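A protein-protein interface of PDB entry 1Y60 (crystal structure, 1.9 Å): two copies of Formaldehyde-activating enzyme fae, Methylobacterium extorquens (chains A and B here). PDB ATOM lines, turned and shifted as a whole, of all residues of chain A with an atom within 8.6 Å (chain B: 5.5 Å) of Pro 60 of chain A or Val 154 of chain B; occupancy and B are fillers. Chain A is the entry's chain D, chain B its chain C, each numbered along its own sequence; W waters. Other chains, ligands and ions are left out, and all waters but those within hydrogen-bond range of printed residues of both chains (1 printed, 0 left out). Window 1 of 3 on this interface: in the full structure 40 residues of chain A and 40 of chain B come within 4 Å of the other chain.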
ATOM      1  N   LEU A  52     -12.755  34.898 -12.684  1.00  0.00           N
ATOM      2  CA  LEU A  52     -13.350  33.583 -12.947  1.00  0.00           C
ATOM      3  C   LEU A  52     -14.711  33.826 -13.586  1.00  0.00           C
ATOM      4  O   LEU A  52     -15.428  34.747 -13.193  1.00  0.00           O
ATOM      5  CB  LEU A  52     -13.591  32.806 -11.655  1.00  0.00           C
ATOM      6  CG  LEU A  52     -12.378  32.389 -10.841  1.00  0.00           C
ATOM      7  CD1 LEU A  52     -12.848  31.905  -9.477  1.00  0.00           C
ATOM      8  CD2 LEU A  52     -11.592  31.303 -11.595  1.00  0.00           C
ATOM      9  N   ALA A  53     -15.074  33.028 -14.576  1.00  0.00           N
ATOM     10  CA  ALA A  53     -16.400  33.197 -15.167  1.00  0.00           C
ATOM     11  C   ALA A  53     -17.399  32.542 -14.199  1.00  0.00           C
ATOM     12  O   ALA A  53     -17.182  31.414 -13.748  1.00  0.00           O
ATOM     13  CB  ALA A  53     -16.474  32.510 -16.523  1.00  0.00           C
ATOM     14  N   VAL A  54     -18.464  33.261 -13.855  1.00  0.00           N
ATOM     15  CA  VAL A  54     -19.489  32.706 -12.976  1.00  0.00           C
ATOM     16  C   VAL A  54     -20.850  32.890 -13.630  1.00  0.00           C
ATOM     17  O   VAL A  54     -21.093  33.900 -14.305  1.00  0.00           O
ATOM     18  CB  VAL A  54     -19.550  33.408 -11.586  1.00  0.00           C
ATOM     19  CG1 VAL A  54     -18.191  33.333 -10.882  1.00  0.00           C
ATOM     20  CG2 VAL A  54     -20.028  34.836 -11.744  1.00  0.00           C
ATOM     21  N   ILE A  55     -21.721  31.903 -13.438  1.00  0.00           N
ATOM     22  CA  ILE A  55     -23.086  31.958 -13.953  1.00  0.00           C
ATOM     23  C   ILE A  55     -23.721  33.096 -13.155  1.00  0.00           C
ATOM     24  O   ILE A  55     -24.504  33.894 -13.681  1.00  0.00           O
ATOM     25  CB  ILE A  55     -23.798  30.620 -13.707  1.00  0.00           C
ATOM     26  CG1 ILE A  55     -23.190  29.573 -14.645  1.00  0.00           C
ATOM     27  CG2 ILE A  55     -25.316  30.745 -13.945  1.00  0.00           C
ATOM     28  CD1 ILE A  55     -23.717  28.192 -14.452  1.00  0.00           C
ATOM     29  N   ALA A  56     -23.327  33.166 -11.885  1.00  0.00           N
ATOM     30  CA  ALA A  56     -23.761  34.207 -10.957  1.00  0.00           C
ATOM     31  C   ALA A  56     -22.822  34.150  -9.744  1.00  0.00           C
ATOM     32  O   ALA A  56     -22.159  33.130  -9.510  1.00  0.00           O
ATOM     33  CB  ALA A  56     -25.210  33.957 -10.517  1.00  0.00           C
ATOM     34  N   PRO A  57     -22.727  35.246  -8.973  1.00  0.00           N
ATOM     35  CA  PRO A  57     -21.846  35.209  -7.802  1.00  0.00           C
ATOM     36  C   PRO A  57     -22.262  33.991  -6.976  1.00  0.00           C
ATOM     37  O   PRO A  57     -23.452  33.719  -6.833  1.00  0.00           O
ATOM     38  CB  PRO A  57     -22.161  36.522  -7.102  1.00  0.00           C
ATOM     39  CG  PRO A  57     -22.418  37.446  -8.264  1.00  0.00           C
ATOM     40  CD  PRO A  57     -23.292  36.592  -9.172  1.00  0.00           C
ATOM     41  N   ASN A  58     -21.281  33.271  -6.452  1.00  0.00           N
ATOM     42  CA  ASN A  58     -21.490  32.061  -5.673  1.00  0.00           C
ATOM     43  C   ASN A  58     -21.898  30.868  -6.513  1.00  0.00           C
ATOM     44  O   ASN A  58     -22.295  29.833  -5.992  1.00  0.00           O
ATOM     45  CB  ASN A  58     -22.460  32.310  -4.513  1.00  0.00           C
ATOM     46  CG  ASN A  58     -21.838  33.201  -3.449  1.00  0.00           C
ATOM     47  OD1 ASN A  58     -20.727  32.923  -2.971  1.00  0.00           O
ATOM     48  ND2 ASN A  58     -22.528  34.279  -3.080  1.00  0.00           N
ATOM     49  N   LEU A  59     -21.795  31.006  -7.827  1.00  0.00           N
ATOM     50  CA  LEU A  59     -22.081  29.882  -8.699  1.00  0.00           C
ATOM     51  C   LEU A  59     -21.178  29.930  -9.941  1.00  0.00           C
ATOM     52  O   LEU A  59     -21.627  30.253 -11.048  1.00  0.00           O
ATOM     53  CB  LEU A  59     -23.562  29.832  -9.124  1.00  0.00           C
ATOM     54  CG  LEU A  59     -23.899  28.472  -9.761  1.00  0.00           C
ATOM     55  CD1 LEU A  59     -23.878  27.434  -8.659  1.00  0.00           C
ATOM     56  CD2 LEU A  59     -25.247  28.456 -10.469  1.00  0.00           C
ATOM     57  N   PRO A  60     -19.883  29.610  -9.767  1.00  0.00           N
ATOM     58  CA  PRO A  60     -18.971  29.628 -10.909  1.00  0.00           C
ATOM     59  C   PRO A  60     -19.264  28.448 -11.827  1.00  0.00           C
ATOM     60  O   PRO A  60     -19.770  27.417 -11.380  1.00  0.00           O
ATOM     61  CB  PRO A  60     -17.606  29.512 -10.248  1.00  0.00           C
ATOM     62  CG  PRO A  60     -17.901  28.657  -9.052  1.00  0.00           C
ATOM     63  CD  PRO A  60     -19.160  29.297  -8.526  1.00  0.00           C
ATOM     64  N   CYS A  61     -18.977  28.597 -13.113  1.00  0.00           N
ATOM     65  CA  CYS A  61     -19.204  27.487 -14.011  1.00  0.00           C
ATOM     66  C   CYS A  61     -18.059  26.524 -13.807  1.00  0.00           C
ATOM     67  O   CYS A  61     -16.993  26.912 -13.327  1.00  0.00           O
ATOM     68  CB  CYS A  61     -19.264  27.949 -15.471  1.00  0.00           C
ATOM     69  SG  CYS A  61     -17.818  28.801 -16.153  1.00  0.00           S
ATOM     70  N   LYS A  62     -18.292  25.257 -14.117  1.00  0.00           N
ATOM     71  CA  LYS A  62     -17.255  24.241 -13.995  1.00  0.00           C
ATOM     72  C   LYS A  62     -17.366  23.504 -15.318  1.00  0.00           C
ATOM     73  O   LYS A  62     -18.471  23.112 -15.712  1.00  0.00           O
ATOM     74  CB  LYS A  62     -17.530  23.274 -12.826  1.00  0.00           C
ATOM     75  CG  LYS A  62     -17.309  23.838 -11.414  1.00  0.00           C
ATOM     76  CD  LYS A  62     -15.881  24.387 -11.233  1.00  0.00           C
ATOM     77  CE  LYS A  62     -15.599  24.863  -9.796  1.00  0.00           C
ATOM     78  NZ  LYS A  62     -15.422  23.723  -8.853  1.00  0.00           N
ATOM     79  N   PRO A  63     -16.230  23.225 -15.980  1.00  0.00           N
ATOM     80  CA  PRO A  63     -14.848  23.525 -15.591  1.00  0.00           C
ATOM     81  C   PRO A  63     -14.483  24.967 -15.273  1.00  0.00           C
ATOM     82  O   PRO A  63     -15.038  25.911 -15.841  1.00  0.00           O
ATOM     83  CB  PRO A  63     -14.029  22.968 -16.753  1.00  0.00           C
ATOM     84  CG  PRO A  63     -14.956  23.135 -17.938  1.00  0.00           C
ATOM     85  CD  PRO A  63     -16.286  22.690 -17.352  1.00  0.00           C
ATOM     86  N   ASN A  64     -13.532  25.116 -14.352  1.00  0.00           N
ATOM     87  CA  ASN A  64     -13.017  26.426 -13.953  1.00  0.00           C
ATOM     88  C   ASN A  64     -12.683  27.245 -15.185  1.00  0.00           C
ATOM     89  O   ASN A  64     -11.960  26.792 -16.065  1.00  0.00           O
ATOM     90  CB  ASN A  64     -11.763  26.252 -13.086  1.00  0.00           C
ATOM     91  CG  ASN A  64     -12.077  25.653 -11.739  1.00  0.00           C
ATOM     92  OD1 ASN A  64     -12.886  26.195 -10.987  1.00  0.00           O
ATOM     93  ND2 ASN A  64     -11.437  24.522 -11.420  1.00  0.00           N
ATOM     94  N   THR A  65     -13.203  28.458 -15.251  1.00  0.00           N
ATOM     95  CA  THR A  65     -12.965  29.271 -16.433  1.00  0.00           C
ATOM     96  C   THR A  65     -12.423  30.641 -16.098  1.00  0.00           C
ATOM     97  O   THR A  65     -12.952  31.297 -15.206  1.00  0.00           O
ATOM     98  CB  THR A  65     -14.278  29.454 -17.223  1.00  0.00           C
ATOM     99  OG1 THR A  65     -14.812  28.183 -17.550  1.00  0.00           O
ATOM    100  CG2 THR A  65     -14.042  30.230 -18.469  1.00  0.00           C
ATOM    101  N   GLN A  87     -20.066  37.893 -19.159  1.00  0.00           N
ATOM    102  CA  GLN A  87     -19.687  36.856 -18.203  1.00  0.00           C
ATOM    103  C   GLN A  87     -20.775  35.797 -18.077  1.00  0.00           C
ATOM    104  O   GLN A  87     -20.504  34.586 -18.152  1.00  0.00           O
ATOM    105  CB  GLN A  87     -19.388  37.459 -16.826  1.00  0.00           C
ATOM    106  CG  GLN A  87     -19.115  36.420 -15.744  1.00  0.00           C
ATOM    107  CD  GLN A  87     -18.733  37.051 -14.423  1.00  0.00           C
ATOM    108  OE1 GLN A  87     -17.790  36.617 -13.762  1.00  0.00           O
ATOM    109  NE2 GLN A  87     -19.458  38.076 -14.028  1.00  0.00           N
ATOM    110  N   ALA A  91     -20.158  31.941 -19.103  1.00  0.00           N
ATOM    111  CA  ALA A  91     -20.361  30.926 -18.088  1.00  0.00           C
ATOM    112  C   ALA A  91     -21.469  29.932 -18.454  1.00  0.00           C
ATOM    113  O   ALA A  91     -21.300  28.718 -18.288  1.00  0.00           O
ATOM    114  CB  ALA A  91     -20.653  31.591 -16.757  1.00  0.00           C
ATOM    115  N   MET A  92     -22.595  30.436 -18.948  1.00  0.00           N
ATOM    116  CA  MET A  92     -23.693  29.551 -19.342  1.00  0.00           C
ATOM    117  C   MET A  92     -23.287  28.660 -20.510  1.00  0.00           C
ATOM    118  O   MET A  92     -23.716  27.498 -20.594  1.00  0.00           O
ATOM    119  CB  MET A  92     -24.940  30.356 -19.731  1.00  0.00           C
ATOM    120  CG  MET A  92     -25.814  30.811 -18.549  1.00  0.00           C
ATOM    121  SD  MET A  92     -26.748  29.499 -17.646  1.00  0.00           S
ATOM    122  CE  MET A  92     -26.806  28.255 -18.784  1.00  0.00           C
ATOM    123  N   VAL A  94     -20.312  27.522 -21.106  1.00  0.00           N
ATOM    124  CA  VAL A  94     -19.477  26.459 -20.563  1.00  0.00           C
ATOM    125  C   VAL A  94     -20.360  25.407 -19.897  1.00  0.00           C
ATOM    126  O   VAL A  94     -20.210  24.211 -20.159  1.00  0.00           O
ATOM    127  CB  VAL A  94     -18.456  27.006 -19.514  1.00  0.00           C
ATOM    128  CG1 VAL A  94     -17.690  25.828 -18.856  1.00  0.00           C
ATOM    129  CG2 VAL A  94     -17.446  27.945 -20.211  1.00  0.00           C
ATOM    130  N   GLN A  95     -21.287  25.844 -19.047  1.00  0.00           N
ATOM    131  CA  GLN A  95     -22.160  24.902 -18.346  1.00  0.00           C
ATOM    132  C   GLN A  95     -23.113  24.158 -19.281  1.00  0.00           C
ATOM    133  O   GLN A  95     -23.375  22.973 -19.084  1.00  0.00           O
ATOM    134  CB  GLN A  95     -22.941  25.595 -17.231  1.00  0.00           C
ATOM    135  CG  GLN A  95     -23.049  24.732 -15.989  1.00  0.00           C
ATOM    136  CD  GLN A  95     -21.667  24.291 -15.504  1.00  0.00           C
ATOM    137  OE1 GLN A  95     -20.781  25.122 -15.304  1.00  0.00           O
ATOM    138  NE2 GLN A  95     -21.480  22.981 -15.319  1.00  0.00           N
ATOM    139  N   ASP A  96     -23.604  24.835 -20.311  1.00  0.00           N
ATOM    140  CA  ASP A  96     -24.480  24.157 -21.263  1.00  0.00           C
ATOM    141  C   ASP A  96     -23.675  23.122 -22.050  1.00  0.00           C
ATOM    142  O   ASP A  96     -24.206  22.062 -22.407  1.00  0.00           O
ATOM    143  CB  ASP A  96     -25.119  25.156 -22.238  1.00  0.00           C
ATOM    144  CG  ASP A  96     -26.332  25.900 -21.640  1.00  0.00           C
ATOM    145  OD1 ASP A  96     -26.860  26.764 -22.356  1.00  0.00           O
ATOM    146  OD2 ASP A  96     -26.753  25.636 -20.483  1.00  0.00           O
ATOM    147  N   VAL A  98     -21.270  21.383 -20.912  1.00  0.00           N
ATOM    148  CA  VAL A  98     -21.130  20.229 -20.021  1.00  0.00           C
ATOM    149  C   VAL A  98     -22.453  19.437 -20.007  1.00  0.00           C
ATOM    150  O   VAL A  98     -22.464  18.206 -20.135  1.00  0.00           O
ATOM    151  CB  VAL A  98     -20.802  20.644 -18.563  1.00  0.00           C
ATOM    152  CG1 VAL A  98     -20.808  19.414 -17.671  1.00  0.00           C
ATOM    153  CG2 VAL A  98     -19.436  21.337 -18.502  1.00  0.00           C
ATOM    154  N   ALA A  99     -23.560  20.162 -19.855  1.00  0.00           N
ATOM    155  CA  ALA A  99     -24.873  19.533 -19.829  1.00  0.00           C
ATOM    156  C   ALA A  99     -25.113  18.754 -21.117  1.00  0.00           C
ATOM    157  O   ALA A  99     -25.640  17.645 -21.084  1.00  0.00           O
ATOM    158  CB  ALA A  99     -25.956  20.594 -19.643  1.00  0.00           C
ATOM    159  N   ALA A 108     -15.206  17.463 -16.434  1.00  0.00           N
ATOM    160  CA  ALA A 108     -15.460  18.842 -16.037  1.00  0.00           C
ATOM    161  C   ALA A 108     -14.768  19.365 -14.776  1.00  0.00           C
ATOM    162  O   ALA A 108     -14.471  20.564 -14.684  1.00  0.00           O
ATOM    163  CB  ALA A 108     -16.959  19.061 -15.939  1.00  0.00           C
ATOM    164  N   ASP A 109     -14.502  18.488 -13.811  1.00  0.00           N
ATOM    165  CA  ASP A 109     -13.846  18.906 -12.570  1.00  0.00           C
ATOM    166  C   ASP A 109     -12.318  18.911 -12.677  1.00  0.00           C
ATOM    167  O   ASP A 109     -11.627  19.256 -11.725  1.00  0.00           O
ATOM    168  CB  ASP A 109     -14.284  17.988 -11.409  1.00  0.00           C
ATOM    169  CG  ASP A 109     -15.759  18.152 -11.064  1.00  0.00           C
ATOM    170  OD1 ASP A 109     -16.473  17.129 -10.981  1.00  0.00           O
ATOM    171  OD2 ASP A 109     -16.205  19.309 -10.874  1.00  0.00           O
ATOM    172  N   GLU B  10     -14.442  30.323  -4.883  1.00  0.00           N
ATOM    173  CA  GLU B  10     -14.957  31.678  -5.049  1.00  0.00           C
ATOM    174  C   GLU B  10     -16.141  31.906  -4.139  1.00  0.00           C
ATOM    175  O   GLU B  10     -16.811  30.961  -3.719  1.00  0.00           O
ATOM    176  CB  GLU B  10     -15.241  32.034  -6.536  1.00  0.00           C
ATOM    177  CG  GLU B  10     -16.578  31.964  -7.245  1.00  0.00           C
ATOM    178  CD  GLU B  10     -17.798  32.629  -6.597  1.00  0.00           C
ATOM    179  OE1 GLU B  10     -18.540  31.908  -5.956  1.00  0.00           O
ATOM    180  OE2 GLU B  10     -18.076  33.828  -6.746  1.00  0.00           O
ATOM    181  N   PRO B 149     -18.111  24.288  -6.030  1.00  0.00           N
ATOM    182  CA  PRO B 149     -19.171  23.323  -6.345  1.00  0.00           C
ATOM    183  C   PRO B 149     -18.782  22.352  -7.443  1.00  0.00           C
ATOM    184  O   PRO B 149     -18.167  22.740  -8.434  1.00  0.00           O
ATOM    185  CB  PRO B 149     -20.315  24.214  -6.776  1.00  0.00           C
ATOM    186  CG  PRO B 149     -19.564  25.316  -7.519  1.00  0.00           C
ATOM    187  CD  PRO B 149     -18.478  25.633  -6.502  1.00  0.00           C
ATOM    188  N   LYS B 150     -19.146  21.086  -7.261  1.00  0.00           N
ATOM    189  CA  LYS B 150     -18.842  20.065  -8.245  1.00  0.00           C
ATOM    190  C   LYS B 150     -19.571  20.437  -9.522  1.00  0.00           C
ATOM    191  O   LYS B 150     -20.632  21.070  -9.469  1.00  0.00           O
ATOM    192  CB  LYS B 150     -19.319  18.690  -7.752  1.00  0.00           C
ATOM    193  CG  LYS B 150     -18.420  18.043  -6.694  1.00  0.00           C
ATOM    194  CD  LYS B 150     -16.990  17.855  -7.215  1.00  0.00           C
ATOM    195  CE  LYS B 150     -16.177  16.938  -6.304  1.00  0.00           C
ATOM    196  NZ  LYS B 150     -16.244  17.350  -4.876  1.00  0.00           N
ATOM    197  N   ALA B 151     -19.007  20.042 -10.663  1.00  0.00           N
ATOM    198  CA  ALA B 151     -19.596  20.336 -11.961  1.00  0.00           C
ATOM    199  C   ALA B 151     -21.039  19.830 -12.043  1.00  0.00           C
ATOM    200  O   ALA B 151     -21.932  20.565 -12.500  1.00  0.00           O
ATOM    201  CB  ALA B 151     -18.747  19.724 -13.083  1.00  0.00           C
ATOM    202  N   SER B 152     -21.281  18.602 -11.587  1.00  0.00           N
ATOM    203  CA  SER B 152     -22.632  18.053 -11.650  1.00  0.00           C
ATOM    204  C   SER B 152     -23.615  18.936 -10.897  1.00  0.00           C
ATOM    205  O   SER B 152     -24.759  19.106 -11.335  1.00  0.00           O
ATOM    206  CB  SER B 152     -22.686  16.625 -11.092  1.00  0.00           C
ATOM    207  OG  SER B 152     -22.456  16.604  -9.703  1.00  0.00           O
ATOM    208  N   VAL B 153     -23.176  19.505  -9.775  1.00  0.00           N
ATOM    209  CA  VAL B 153     -24.039  20.394  -8.989  1.00  0.00           C
ATOM    210  C   VAL B 153     -24.309  21.717  -9.719  1.00  0.00           C
ATOM    211  O   VAL B 153     -25.428  22.249  -9.677  1.00  0.00           O
ATOM    212  CB  VAL B 153     -23.428  20.692  -7.574  1.00  0.00           C
ATOM    213  CG1 VAL B 153     -24.230  21.798  -6.869  1.00  0.00           C
ATOM    214  CG2 VAL B 153     -23.474  19.420  -6.708  1.00  0.00           C
ATOM    215  N   VAL B 154     -23.303  22.263 -10.394  1.00  0.00           N
ATOM    216  CA  VAL B 154     -23.516  23.514 -11.110  1.00  0.00           C
ATOM    217  C   VAL B 154     -24.447  23.269 -12.290  1.00  0.00           C
ATOM    218  O   VAL B 154     -25.330  24.079 -12.579  1.00  0.00           O
ATOM    219  CB  VAL B 154     -22.195  24.134 -11.652  1.00  0.00           C
ATOM    220  CG1 VAL B 154     -22.488  25.516 -12.246  1.00  0.00           C
ATOM    221  CG2 VAL B 154     -21.174  24.281 -10.524  1.00  0.00           C
ATOM    222  N   THR B 155     -24.250  22.148 -12.971  1.00  0.00           N
ATOM    223  CA  THR B 155     -25.080  21.800 -14.115  1.00  0.00           C
ATOM    224  C   THR B 155     -26.550  21.712 -13.713  1.00  0.00           C
ATOM    225  O   THR B 155     -27.414  22.245 -14.401  1.00  0.00           O
ATOM    226  CB  THR B 155     -24.643  20.454 -14.735  1.00  0.00           C
ATOM    227  OG1 THR B 155     -23.325  20.609 -15.269  1.00  0.00           O
ATOM    228  CG2 THR B 155     -25.581  20.046 -15.885  1.00  0.00           C
ATOM    229  N   GLU B 156     -26.818  21.041 -12.596  1.00  0.00           N
ATOM    230  CA  GLU B 156     -28.173  20.886 -12.088  1.00  0.00           C
ATOM    231  C   GLU B 156     -28.864  22.221 -11.786  1.00  0.00           C
ATOM    232  O   GLU B 156     -30.055  22.389 -12.057  1.00  0.00           O
ATOM    233  CB  GLU B 156     -28.170  20.047 -10.809  1.00  0.00           C
ATOM    234  CG  GLU B 156     -28.128  18.539 -11.007  1.00  0.00           C
ATOM    235  CD  GLU B 156     -27.964  17.786  -9.683  1.00  0.00           C
ATOM    236  OE1 GLU B 156     -28.604  18.193  -8.687  1.00  0.00           O
ATOM    237  OE2 GLU B 156     -27.210  16.784  -9.638  1.00  0.00           O
ATOM    238  N   GLN B 157     -28.138  23.190 -11.241  1.00  0.00           N
ATOM    239  CA  GLN B 157     -28.802  24.435 -10.898  1.00  0.00           C
ATOM    240  C   GLN B 157     -28.454  25.654 -11.734  1.00  0.00           C
ATOM    241  O   GLN B 157     -28.751  26.783 -11.342  1.00  0.00           O
ATOM    242  CB  GLN B 157     -28.588  24.732  -9.413  1.00  0.00           C
ATOM    243  CG  GLN B 157     -27.174  25.014  -9.018  1.00  0.00           C
ATOM    244  CD  GLN B 157     -27.015  25.042  -7.515  1.00  0.00           C
ATOM    245  OE1 GLN B 157     -27.031  23.995  -6.861  1.00  0.00           O
ATOM    246  NE2 GLN B 157     -26.877  26.240  -6.954  1.00  0.00           N
ATOM    247  N   ARG B 158     -27.872  25.438 -12.909  1.00  0.00           N
ATOM    248  CA  ARG B 158     -27.490  26.567 -13.754  1.00  0.00           C
ATOM    249  C   ARG B 158     -28.651  27.444 -14.183  1.00  0.00           C
ATOM    250  O   ARG B 158     -28.524  28.662 -14.242  1.00  0.00           O
ATOM    251  CB  ARG B 158     -26.731  26.083 -14.994  1.00  0.00           C
ATOM    252  CG  ARG B 158     -27.515  25.233 -15.976  1.00  0.00           C
ATOM    253  CD  ARG B 158     -26.544  24.601 -16.970  1.00  0.00           C
ATOM    254  NE  ARG B 158     -27.198  24.059 -18.150  1.00  0.00           N
ATOM    255  CZ  ARG B 158     -27.992  22.995 -18.145  1.00  0.00           C
ATOM    256  NH1 ARG B 158     -28.223  22.355 -17.021  1.00  0.00           N
ATOM    257  NH2 ARG B 158     -28.570  22.578 -19.263  1.00  0.00           N
HETATM  258  O   HOH W   1     -19.209  16.763 -11.064  1.00  0.00           O
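Water W1 lies within hydrogen-bond range of OD1 of Asp 109 of chain A (2.8 Å), N of Ser 152 of chain B (2.8 Å) and N of Ala 151 of chain B (3.3 Å).
The side-chain carboxylate of Glu 10 of chain B lies close to the backbone NH of Asn 58 of chain A (3.1 Å).
NZ of Lys 62 of chain A sits at hydrogen-bond distance from O of Pro 149 of chain B (2.9 Å).
N of Ala 151 of chain B lies within hydrogen-bond range of OD2 of Asp 109 of chain A (2.9 Å).
NE2 of Gln 95 of chain A sits at hydrogen-bond distance from OG1 of Thr 155 of chain B, at 3.0 Å.
NE of Arg 158 of chain B is in salt-bridge range of OD2 of Asp 96 of chain A (2.9 Å).
O of Ala 151 of chain B is in hydrogen-bond range of OG1 of Thr 155 of chain B, 3.1 Å away.
O of Thr 155 of chain B lies within hydrogen-bond range of NH1 of Arg 158 of chain B, 2.7 Å away.
The side-chain amide oxygen (OE1) of Gln 87 of chain A sits close to the backbone carbonyl oxygen (O) of Leu 52 of chain A (3.1 Å).
N of Lys 62 of chain A sits at hydrogen-bond distance from OE1 of Gln 95 of chain A (2.8 Å).
Leu 52 of chain A touches Glu 10 of chain B.
CG1 of Val 154 of chain B touches CD1 of Ile 55 of chain A (3.7 Å).
Leu 59 of chain A touches Gln 157 of chain B.
CD of Pro 60 of chain A touches OE1 of Glu 10 of chain B, 3.7 Å away.
CG of Pro 60 of chain A touches CD of Pro 149 of chain B (3.997 Å).
O of Pro 60 of chain A touches CG1 of Val 154 of chain B, at 3.4 Å.
Lys 62 of chain A touches Ala 151 of chain B.
Met 92 of chain A touches Arg 158 of chain B.
Gln 95 of chain A touches Val 154 of chain B.
Asp 109 of chain A touches Lys 150 of chain B (OD2 to C, 3.8 Å).
Of the 11 printed residues of chain B, 8 touch a printed residue of chain A.
Hydrophobic or aromatic side chains of chain B that line the printed part of chain A: Pro 149, Ala 151 and Val 154.
Along chain B the printed residues that touch a printed residue of chain A span positions 10 to 158.
Of the 24 printed residues of chain A, 13 touch a printed residue of chain B.
Printed residues of chain A that touch a printed residue of chain B: Leu 52, Ile 55, Asn 58, Leu 59, Pro 60, Lys 62, Met 92, Gln 95, Asp 96, Val 98, Ala 99, Ala 108 and Asp 109.
Hydrophobic or aromatic side chains of chain A that line the printed part of chain B: Leu 52, Ile 55, Leu 59, Pro 60, Met 92, Val 98, Ala 99 and Ala 108.
Among the printed residues, 24 pairs touch across the chains.
Among the printed residues, Asp or Glu carboxylates within 4 Å of a Lys or Arg side-chain nitrogen of the other chain: Asp 96 of chain A with Arg 158 of chain B.
Printed residues of chain B within 4 Å of Pro 60 of chain A: Glu 10, Pro 149 and Val 154.
Of the printed residues of chain A, Val 154 of chain B touches Ile 55 (3.7 Å), Pro 60 (3.4 Å), Lys 62 (3.99 Å) and Gln 95 (3.5 Å).
Of the printed residues of chain B, Asp 96 of chain A touches Arg 158 (2.9 Å).
Of the printed residues of chain B, Leu 52 of chain A touches Glu 10 (3.8 Å).
Of the printed residues of chain A, Ala 151 of chain B touches Lys 62, Gln 95, Ala 108 and Asp 109.
The nearest printed residue of chain A that does not touch Val 154 of chain B is Leu 59 of chain A (4.1 Å).
No position is printed for both chains.
Of the 24 pairs that touch across the chains among the printed residues, none has its exchanged pair printed and touching as well.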
